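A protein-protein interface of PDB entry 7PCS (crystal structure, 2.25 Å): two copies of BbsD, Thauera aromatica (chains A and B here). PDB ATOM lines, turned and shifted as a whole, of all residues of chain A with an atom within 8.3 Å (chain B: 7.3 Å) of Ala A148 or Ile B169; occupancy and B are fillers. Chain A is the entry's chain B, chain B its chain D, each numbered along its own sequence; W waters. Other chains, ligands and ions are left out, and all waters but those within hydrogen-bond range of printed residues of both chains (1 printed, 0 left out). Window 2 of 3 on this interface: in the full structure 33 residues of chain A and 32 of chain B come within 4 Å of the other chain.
Water W1 lies within hydrogen-bond range of the side-chain hydroxyl of Thr A151 (2.7 Å), the side-chain carboxylate of Glu B170 (2.7 Å), the backbone carbonyl oxygen of Gly A96 (2.8 Å) and the backbone NH of Gln A150 (3.5 Å).
Among the printed residues, pairs that only touch across the chains: Ala A97 with Glu B170 (3.7 Å), Gly A146 with Arg B165 (3.8 Å), Gly A146 with Ala B166 (3.6 Å), Gly A146 with Ile B169 (3.5 Å), Gly A147 with Ala B166 (3.6 Å), Ala A148 with Ile B169 (3.9 Å), Ala A148 with Glu B170 (3.96 Å), Thr A151 with Met B163 (3.6 Å), Thr A151 with Leu B167 (3.1 Å) and Ser A154 with Ala B166 (3.8 Å).
The backbone carbonyl oxygen (O) of Gln A150 lies close to the side-chain hydroxyl (OG) of Ser A154. O of Gly A149 is in hydrogen-bond range of N of Gly A96, 2.8 Å away. OG of Ser A154 lies within hydrogen-bond range of O of Ala A143, 2.6 Å away. O of Gly A146 sits at hydrogen-bond distance from NH2 of Arg A142, 3.1 Å away. N of Gly A147 is in hydrogen-bond range of OG of Ser A154.
No position is printed for both chains. Of the 13 pairs that touch across the chains among the printed residues, none has its exchanged pair printed and touching as well.
Ile B169 touches two residues of chain A. Printed residues of chain B within 4 Å of Gly A147: Ala B166 (3.6 Å). Of the printed residues of chain A, Leu B167 touches Thr A151. Printed residues of chain A within 4 Å of Arg B165: Leu A145 (2.8 Å) and Gly A146 (3.8 Å). Val B178 touches none of the printed residues of chain A. Thr B233 touches none of the printed residues of chain A. The nearest residue of chain B that does not touch Ala A148 is Ala B166 (4.2 Å). The nearest residue of chain A that does not touch Ile B169 is Gly A147 (4.5 Å). The nearest printed residue of chain B that does not touch Thr A151 is Glu B170 (4.2 Å).
The side-chain carboxylate (OE1) of Glu B170 lies within hydrogen-bond range of the backbone NH (N) of Gly A149 (2.8 Å). The guanidinium group of Arg B165 lies within hydrogen-bond range of the backbone carbonyl oxygen of Leu A145, 2.8 Å away. The backbone NH of Leu A98 sits at hydrogen-bond distance from the side-chain carboxylate of Glu B170 (2.8 Å).
Hydrophobic or aromatic side chains of chain B that line the printed part of chain A: Met B163, Ala B166, Leu B167 and Ile B169. Of the 18 printed residues of chain A, 9 touch a printed residue of chain B. Among the printed residues, 13 pairs touch across the chains. Among the printed residues, no Asp or Glu carboxylate lies within 4 Å of a Lys or Arg side-chain nitrogen of the other chain.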
ATOM      1  N   GLU A  93     -12.765 -18.804  12.365  1.00  0.00           N
ATOM      2  CA  GLU A  93     -11.650 -18.982  13.284  1.00  0.00           C
ATOM      3  C   GLU A  93     -10.470 -19.659  12.599  1.00  0.00           C
ATOM      4  O   GLU A  93     -10.644 -20.633  11.860  1.00  0.00           O
ATOM      5  CB  GLU A  93     -12.073 -19.807  14.509  1.00  0.00           C
ATOM      6  CG  GLU A  93     -10.909 -20.272  15.374  1.00  0.00           C
ATOM      7  CD  GLU A  93     -11.349 -20.864  16.701  1.00  0.00           C
ATOM      8  OE1 GLU A  93     -12.448 -21.455  16.751  1.00  0.00           O
ATOM      9  OE2 GLU A  93     -10.602 -20.735  17.694  1.00  0.00           O
ATOM     10  N   ALA A  95      -7.129 -21.245  14.465  1.00  0.00           N
ATOM     11  CA  ALA A  95      -6.627 -21.593  15.780  1.00  0.00           C
ATOM     12  C   ALA A  95      -5.305 -22.329  15.627  1.00  0.00           C
ATOM     13  O   ALA A  95      -4.892 -22.690  14.524  1.00  0.00           O
ATOM     14  CB  ALA A  95      -7.639 -22.455  16.539  1.00  0.00           C
ATOM     15  N   GLY A  96      -4.640 -22.528  16.747  1.00  0.00           N
ATOM     16  CA  GLY A  96      -3.350 -23.183  16.794  1.00  0.00           C
ATOM     17  C   GLY A  96      -2.546 -22.666  17.966  1.00  0.00           C
ATOM     18  O   GLY A  96      -2.818 -21.613  18.544  1.00  0.00           O
ATOM     19  N   ALA A  97      -1.532 -23.438  18.338  1.00  0.00           N
ATOM     20  CA  ALA A  97      -0.613 -22.992  19.370  1.00  0.00           C
ATOM     21  C   ALA A  97      -0.118 -21.595  19.036  1.00  0.00           C
ATOM     22  O   ALA A  97       0.017 -21.226  17.866  1.00  0.00           O
ATOM     23  CB  ALA A  97       0.566 -23.959  19.489  1.00  0.00           C
ATOM     24  N   LEU A  98       0.155 -20.814  20.082  1.00  0.00           N
ATOM     25  CA  LEU A  98       0.582 -19.433  19.889  1.00  0.00           C
ATOM     26  C   LEU A  98       1.718 -19.350  18.877  1.00  0.00           C
ATOM     27  O   LEU A  98       1.704 -18.506  17.972  1.00  0.00           O
ATOM     28  CB  LEU A  98       1.009 -18.831  21.225  1.00  0.00           C
ATOM     29  CG  LEU A  98       1.490 -17.380  21.188  1.00  0.00           C
ATOM     30  CD1 LEU A  98       0.450 -16.472  20.545  1.00  0.00           C
ATOM     31  CD2 LEU A  98       1.818 -16.912  22.604  1.00  0.00           C
ATOM     32  N   ARG A 142     -18.553 -18.780  23.938  1.00  0.00           N
ATOM     33  CA  ARG A 142     -18.005 -19.120  25.240  1.00  0.00           C
ATOM     34  C   ARG A 142     -16.503 -18.870  25.275  1.00  0.00           C
ATOM     35  O   ARG A 142     -15.936 -18.650  26.352  1.00  0.00           O
ATOM     36  CB  ARG A 142     -18.298 -20.584  25.601  1.00  0.00           C
ATOM     37  CG  ARG A 142     -17.978 -20.945  27.044  1.00  0.00           C
ATOM     38  CD  ARG A 142     -17.184 -22.256  27.116  1.00  0.00           C
ATOM     39  NE  ARG A 142     -15.878 -22.137  26.473  1.00  0.00           N
ATOM     40  CZ  ARG A 142     -14.797 -21.636  27.060  1.00  0.00           C
ATOM     41  NH1 ARG A 142     -14.820 -21.213  28.317  1.00  0.00           N
ATOM     42  NH2 ARG A 142     -13.664 -21.547  26.366  1.00  0.00           N
ATOM     43  N   ALA A 143     -15.851 -18.889  24.112  1.00  0.00           N
ATOM     44  CA  ALA A 143     -14.405 -18.763  24.031  1.00  0.00           C
ATOM     45  C   ALA A 143     -13.898 -17.354  24.310  1.00  0.00           C
ATOM     46  O   ALA A 143     -12.679 -17.175  24.400  1.00  0.00           O
ATOM     47  CB  ALA A 143     -13.931 -19.214  22.648  1.00  0.00           C
ATOM     48  N   LEU A 145     -14.164 -16.099  27.085  1.00  0.00           N
ATOM     49  CA  LEU A 145     -13.608 -16.378  28.402  1.00  0.00           C
ATOM     50  C   LEU A 145     -12.224 -16.998  28.333  1.00  0.00           C
ATOM     51  O   LEU A 145     -11.600 -17.218  29.379  1.00  0.00           O
ATOM     52  CB  LEU A 145     -14.557 -17.307  29.160  1.00  0.00           C
ATOM     53  CG  LEU A 145     -15.968 -16.750  29.360  1.00  0.00           C
ATOM     54  CD1 LEU A 145     -16.876 -17.799  30.007  1.00  0.00           C
ATOM     55  CD2 LEU A 145     -15.911 -15.480  30.194  1.00  0.00           C
ATOM     56  N   GLY A 146     -11.738 -17.300  27.136  1.00  0.00           N
ATOM     57  CA  GLY A 146     -10.411 -17.859  26.988  1.00  0.00           C
ATOM     58  C   GLY A 146     -10.394 -19.314  26.568  1.00  0.00           C
ATOM     59  O   GLY A 146     -11.010 -20.166  27.222  1.00  0.00           O
ATOM     60  N   GLY A 147      -9.688 -19.610  25.473  1.00  0.00           N
ATOM     61  CA  GLY A 147      -9.511 -20.981  25.034  1.00  0.00           C
ATOM     62  C   GLY A 147      -8.089 -21.265  24.601  1.00  0.00           C
ATOM     63  O   GLY A 147      -7.529 -20.520  23.797  1.00  0.00           O
ATOM     64  N   ALA A 148      -7.489 -22.326  25.137  1.00  0.00           N
ATOM     65  CA  ALA A 148      -6.143 -22.696  24.729  1.00  0.00           C
ATOM     66  C   ALA A 148      -6.126 -22.955  23.232  1.00  0.00           C
ATOM     67  O   ALA A 148      -7.047 -23.570  22.688  1.00  0.00           O
ATOM     68  CB  ALA A 148      -5.681 -23.938  25.485  1.00  0.00           C
ATOM     69  N   GLY A 149      -5.083 -22.463  22.566  1.00  0.00           N
ATOM     70  CA  GLY A 149      -4.980 -22.578  21.126  1.00  0.00           C
ATOM     71  C   GLY A 149      -5.936 -21.710  20.346  1.00  0.00           C
ATOM     72  O   GLY A 149      -6.057 -21.883  19.129  1.00  0.00           O
ATOM     73  N   GLN A 150      -6.611 -20.772  20.998  1.00  0.00           N
ATOM     74  CA  GLN A 150      -7.599 -19.938  20.330  1.00  0.00           C
ATOM     75  C   GLN A 150      -7.317 -18.460  20.561  1.00  0.00           C
ATOM     76  O   GLN A 150      -8.235 -17.647  20.696  1.00  0.00           O
ATOM     77  CB  GLN A 150      -9.013 -20.278  20.793  1.00  0.00           C
ATOM     78  CG  GLN A 150      -9.463 -21.693  20.552  1.00  0.00           C
ATOM     79  CD  GLN A 150     -10.886 -21.922  21.025  1.00  0.00           C
ATOM     80  OE1 GLN A 150     -11.119 -22.338  22.164  1.00  0.00           O
ATOM     81  NE2 GLN A 150     -11.848 -21.651  20.146  1.00  0.00           N
ATOM     82  N   THR A 151      -6.047 -18.076  20.611  1.00  0.00           N
ATOM     83  CA  THR A 151      -5.726 -16.666  20.827  1.00  0.00           C
ATOM     84  C   THR A 151      -6.500 -15.735  19.905  1.00  0.00           C
ATOM     85  O   THR A 151      -7.110 -14.777  20.405  1.00  0.00           O
ATOM     86  CB  THR A 151      -4.214 -16.455  20.664  1.00  0.00           C
ATOM     87  OG1 THR A 151      -3.505 -17.296  21.579  1.00  0.00           O
ATOM     88  CG2 THR A 151      -3.842 -14.999  20.921  1.00  0.00           C
ATOM     89  N   PRO A 152      -6.538 -15.947  18.587  1.00  0.00           N
ATOM     90  CA  PRO A 152      -7.261 -14.982  17.732  1.00  0.00           C
ATOM     91  C   PRO A 152      -8.764 -14.973  17.979  1.00  0.00           C
ATOM     92  O   PRO A 152      -9.372 -13.899  18.074  1.00  0.00           O
ATOM     93  CB  PRO A 152      -6.920 -15.444  16.305  1.00  0.00           C
ATOM     94  CG  PRO A 152      -5.686 -16.334  16.459  1.00  0.00           C
ATOM     95  CD  PRO A 152      -5.884 -17.010  17.800  1.00  0.00           C
ATOM     96  N   SER A 154     -10.472 -15.991  20.721  1.00  0.00           N
ATOM     97  CA  SER A 154     -10.803 -15.443  22.036  1.00  0.00           C
ATOM     98  C   SER A 154     -10.646 -13.929  22.057  1.00  0.00           C
ATOM     99  O   SER A 154     -11.473 -13.219  22.643  1.00  0.00           O
ATOM    100  CB  SER A 154      -9.936 -16.075  23.126  1.00  0.00           C
ATOM    101  OG  SER A 154     -10.291 -17.428  23.345  1.00  0.00           O
ATOM    102  N   ALA A 247     -15.914 -24.698  32.287  1.00  0.00           N
ATOM    103  CA  ALA A 247     -15.501 -25.325  31.036  1.00  0.00           C
ATOM    104  C   ALA A 247     -14.164 -26.045  31.170  1.00  0.00           C
ATOM    105  O   ALA A 247     -13.411 -26.159  30.200  1.00  0.00           O
ATOM    106  CB  ALA A 247     -15.432 -24.285  29.920  1.00  0.00           C
ATOM    107  N   GLY A 248     -13.857 -26.528  32.364  1.00  0.00           N
ATOM    108  CA  GLY A 248     -12.591 -27.184  32.610  1.00  0.00           C
ATOM    109  C   GLY A 248     -12.695 -28.692  32.699  1.00  0.00           C
ATOM    110  O   GLY A 248     -13.739 -29.275  32.412  1.00  0.00           O
ATOM    111  OXT GLY A 248     -11.735 -29.375  33.052  1.00  0.00           O
ATOM    112  N   MET B 163      -7.624 -12.321  25.287  1.00  0.00           N
ATOM    113  CA  MET B 163      -6.294 -12.857  25.033  1.00  0.00           C
ATOM    114  C   MET B 163      -5.612 -13.251  26.336  1.00  0.00           C
ATOM    115  O   MET B 163      -4.970 -14.306  26.420  1.00  0.00           O
ATOM    116  CB  MET B 163      -5.453 -11.834  24.279  1.00  0.00           C
ATOM    117  CG  MET B 163      -4.400 -12.466  23.390  1.00  0.00           C
ATOM    118  SD  MET B 163      -3.067 -11.338  22.987  1.00  0.00           S
ATOM    119  CE  MET B 163      -3.963 -10.012  22.169  1.00  0.00           C
ATOM    120  N   THR B 164      -5.738 -12.413  27.365  1.00  0.00           N
ATOM    121  CA  THR B 164      -5.121 -12.727  28.648  1.00  0.00           C
ATOM    122  C   THR B 164      -5.611 -14.072  29.160  1.00  0.00           C
ATOM    123  O   THR B 164      -4.819 -14.924  29.580  1.00  0.00           O
ATOM    124  CB  THR B 164      -5.428 -11.619  29.657  1.00  0.00           C
ATOM    125  OG1 THR B 164      -5.059 -10.344  29.105  1.00  0.00           O
ATOM    126  CG2 THR B 164      -4.678 -11.860  30.955  1.00  0.00           C
ATOM    127  N   ARG B 165      -6.924 -14.279  29.114  1.00  0.00           N
ATOM    128  CA  ARG B 165      -7.507 -15.521  29.600  1.00  0.00           C
ATOM    129  C   ARG B 165      -7.065 -16.704  28.751  1.00  0.00           C
ATOM    130  O   ARG B 165      -6.671 -17.748  29.279  1.00  0.00           O
ATOM    131  CB  ARG B 165      -9.027 -15.398  29.598  1.00  0.00           C
ATOM    132  CG  ARG B 165      -9.577 -14.279  30.491  1.00  0.00           C
ATOM    133  CD  ARG B 165     -10.033 -14.810  31.849  1.00  0.00           C
ATOM    134  NE  ARG B 165     -11.226 -15.642  31.719  1.00  0.00           N
ATOM    135  CZ  ARG B 165     -12.109 -15.863  32.685  1.00  0.00           C
ATOM    136  NH1 ARG B 165     -11.967 -15.333  33.891  1.00  0.00           N
ATOM    137  NH2 ARG B 165     -13.154 -16.649  32.440  1.00  0.00           N
ATOM    138  N   ALA B 166      -7.128 -16.562  27.428  1.00  0.00           N
ATOM    139  CA  ALA B 166      -6.748 -17.662  26.550  1.00  0.00           C
ATOM    140  C   ALA B 166      -5.309 -18.093  26.795  1.00  0.00           C
ATOM    141  O   ALA B 166      -5.025 -19.285  26.959  1.00  0.00           O
ATOM    142  CB  ALA B 166      -6.936 -17.250  25.090  1.00  0.00           C
ATOM    143  N   LEU B 167      -4.382 -17.132  26.818  1.00  0.00           N
ATOM    144  CA  LEU B 167      -2.969 -17.463  26.956  1.00  0.00           C
ATOM    145  C   LEU B 167      -2.613 -17.861  28.381  1.00  0.00           C
ATOM    146  O   LEU B 167      -1.676 -18.639  28.578  1.00  0.00           O
ATOM    147  CB  LEU B 167      -2.108 -16.290  26.492  1.00  0.00           C
ATOM    148  CG  LEU B 167      -2.174 -16.076  24.978  1.00  0.00           C
ATOM    149  CD1 LEU B 167      -1.260 -14.952  24.530  1.00  0.00           C
ATOM    150  CD2 LEU B 167      -1.855 -17.364  24.220  1.00  0.00           C
ATOM    151  N   ALA B 168      -3.316 -17.334  29.387  1.00  0.00           N
ATOM    152  CA  ALA B 168      -3.136 -17.863  30.735  1.00  0.00           C
ATOM    153  C   ALA B 168      -3.389 -19.366  30.761  1.00  0.00           C
ATOM    154  O   ALA B 168      -2.646 -20.122  31.397  1.00  0.00           O
ATOM    155  CB  ALA B 168      -4.063 -17.159  31.725  1.00  0.00           C
ATOM    156  N   ILE B 169      -4.439 -19.814  30.071  1.00  0.00           N
ATOM    157  CA  ILE B 169      -4.727 -21.243  30.007  1.00  0.00           C
ATOM    158  C   ILE B 169      -3.646 -21.971  29.218  1.00  0.00           C
ATOM    159  O   ILE B 169      -3.175 -23.041  29.622  1.00  0.00           O
ATOM    160  CB  ILE B 169      -6.120 -21.484  29.392  1.00  0.00           C
ATOM    161  CG1 ILE B 169      -7.220 -20.872  30.265  1.00  0.00           C
ATOM    162  CG2 ILE B 169      -6.374 -22.975  29.194  1.00  0.00           C
ATOM    163  CD1 ILE B 169      -8.607 -20.895  29.630  1.00  0.00           C
ATOM    164  N   GLU B 170      -3.243 -21.415  28.080  1.00  0.00           N
ATOM    165  CA  GLU B 170      -2.366 -22.153  27.182  1.00  0.00           C
ATOM    166  C   GLU B 170      -0.932 -22.217  27.693  1.00  0.00           C
ATOM    167  O   GLU B 170      -0.303 -23.278  27.642  1.00  0.00           O
ATOM    168  CB  GLU B 170      -2.397 -21.515  25.795  1.00  0.00           C
ATOM    169  CG  GLU B 170      -1.478 -22.197  24.763  1.00  0.00           C
ATOM    170  CD  GLU B 170      -1.523 -21.516  23.403  1.00  0.00           C
ATOM    171  OE1 GLU B 170      -2.627 -21.121  22.985  1.00  0.00           O
ATOM    172  OE2 GLU B 170      -0.465 -21.362  22.748  1.00  0.00           O
ATOM    173  N   LEU B 171      -0.397 -21.103  28.180  1.00  0.00           N
ATOM    174  CA  LEU B 171       1.022 -21.002  28.497  1.00  0.00           C
ATOM    175  C   LEU B 171       1.346 -21.422  29.921  1.00  0.00           C
ATOM    176  O   LEU B 171       2.527 -21.481  30.278  1.00  0.00           O
ATOM    177  CB  LEU B 171       1.513 -19.568  28.261  1.00  0.00           C
ATOM    178  CG  LEU B 171       1.166 -18.977  26.895  1.00  0.00           C
ATOM    179  CD1 LEU B 171       1.777 -17.590  26.725  1.00  0.00           C
ATOM    180  CD2 LEU B 171       1.616 -19.908  25.775  1.00  0.00           C
ATOM    181  N   GLY B 172       0.337 -21.731  30.731  1.00  0.00           N
ATOM    182  CA  GLY B 172       0.592 -22.025  32.128  1.00  0.00           C
ATOM    183  C   GLY B 172       1.533 -23.196  32.328  1.00  0.00           C
ATOM    184  O   GLY B 172       2.372 -23.179  33.231  1.00  0.00           O
ATOM    185  N   ARG B 173       1.405 -24.234  31.497  1.00  0.00           N
ATOM    186  CA  ARG B 173       2.225 -25.423  31.685  1.00  0.00           C
ATOM    187  C   ARG B 173       3.699 -25.126  31.476  1.00  0.00           C
ATOM    188  O   ARG B 173       4.548 -25.882  31.955  1.00  0.00           O
ATOM    189  CB  ARG B 173       1.773 -26.532  30.733  1.00  0.00           C
ATOM    190  CG  ARG B 173       1.839 -26.144  29.267  1.00  0.00           C
ATOM    191  CD  ARG B 173       0.690 -26.751  28.454  1.00  0.00           C
ATOM    192  NE  ARG B 173       0.645 -28.209  28.403  1.00  0.00           N
ATOM    193  CZ  ARG B 173      -0.483 -28.905  28.406  1.00  0.00           C
ATOM    194  NH1 ARG B 173      -1.663 -28.309  28.501  1.00  0.00           N
ATOM    195  NH2 ARG B 173      -0.429 -30.230  28.308  1.00  0.00           N
ATOM    196  N   ILE B 176       4.570 -19.848  32.517  1.00  0.00           N
ATOM    197  CA  ILE B 176       4.266 -18.478  32.129  1.00  0.00           C
ATOM    198  C   ILE B 176       2.895 -18.113  32.682  1.00  0.00           C
ATOM    199  O   ILE B 176       1.911 -18.823  32.435  1.00  0.00           O
ATOM    200  CB  ILE B 176       4.296 -18.309  30.600  1.00  0.00           C
ATOM    201  CG1 ILE B 176       5.670 -18.690  30.045  1.00  0.00           C
ATOM    202  CG2 ILE B 176       3.927 -16.885  30.220  1.00  0.00           C
ATOM    203  CD1 ILE B 176       5.750 -18.659  28.523  1.00  0.00           C
ATOM    204  N   VAL B 178      -0.088 -15.061  32.711  1.00  0.00           N
ATOM    205  CA  VAL B 178      -0.604 -14.026  31.826  1.00  0.00           C
ATOM    206  C   VAL B 178      -1.727 -13.330  32.579  1.00  0.00           C
ATOM    207  O   VAL B 178      -2.770 -13.940  32.850  1.00  0.00           O
ATOM    208  CB  VAL B 178      -1.100 -14.599  30.491  1.00  0.00           C
ATOM    209  CG1 VAL B 178      -1.440 -13.481  29.514  1.00  0.00           C
ATOM    210  CG2 VAL B 178      -0.059 -15.547  29.906  1.00  0.00           C
ATOM    211  N   THR B 233      -2.613 -16.071  37.681  1.00  0.00           N
ATOM    212  CA  THR B 233      -2.636 -15.971  36.228  1.00  0.00           C
ATOM    213  C   THR B 233      -4.082 -15.911  35.757  1.00  0.00           C
ATOM    214  O   THR B 233      -4.997 -16.375  36.445  1.00  0.00           O
ATOM    215  CB  THR B 233      -1.890 -17.147  35.582  1.00  0.00           C
ATOM    216  OG1 THR B 233      -1.662 -16.880  34.192  1.00  0.00           O
ATOM    217  CG2 THR B 233      -2.672 -18.432  35.729  1.00  0.00           C
ATOM    218  N   GLY B 234      -4.277 -15.311  34.587  1.00  0.00           N
ATOM    219  CA  GLY B 234      -5.609 -15.154  34.044  1.00  0.00           C
ATOM    220  C   GLY B 234      -6.437 -14.065  34.683  1.00  0.00           C
ATOM    221  O   GLY B 234      -7.659 -14.053  34.505  1.00  0.00           O
HETATM  222  O   HOH W   1      -3.302 -19.830  20.653  1.00  0.00           O
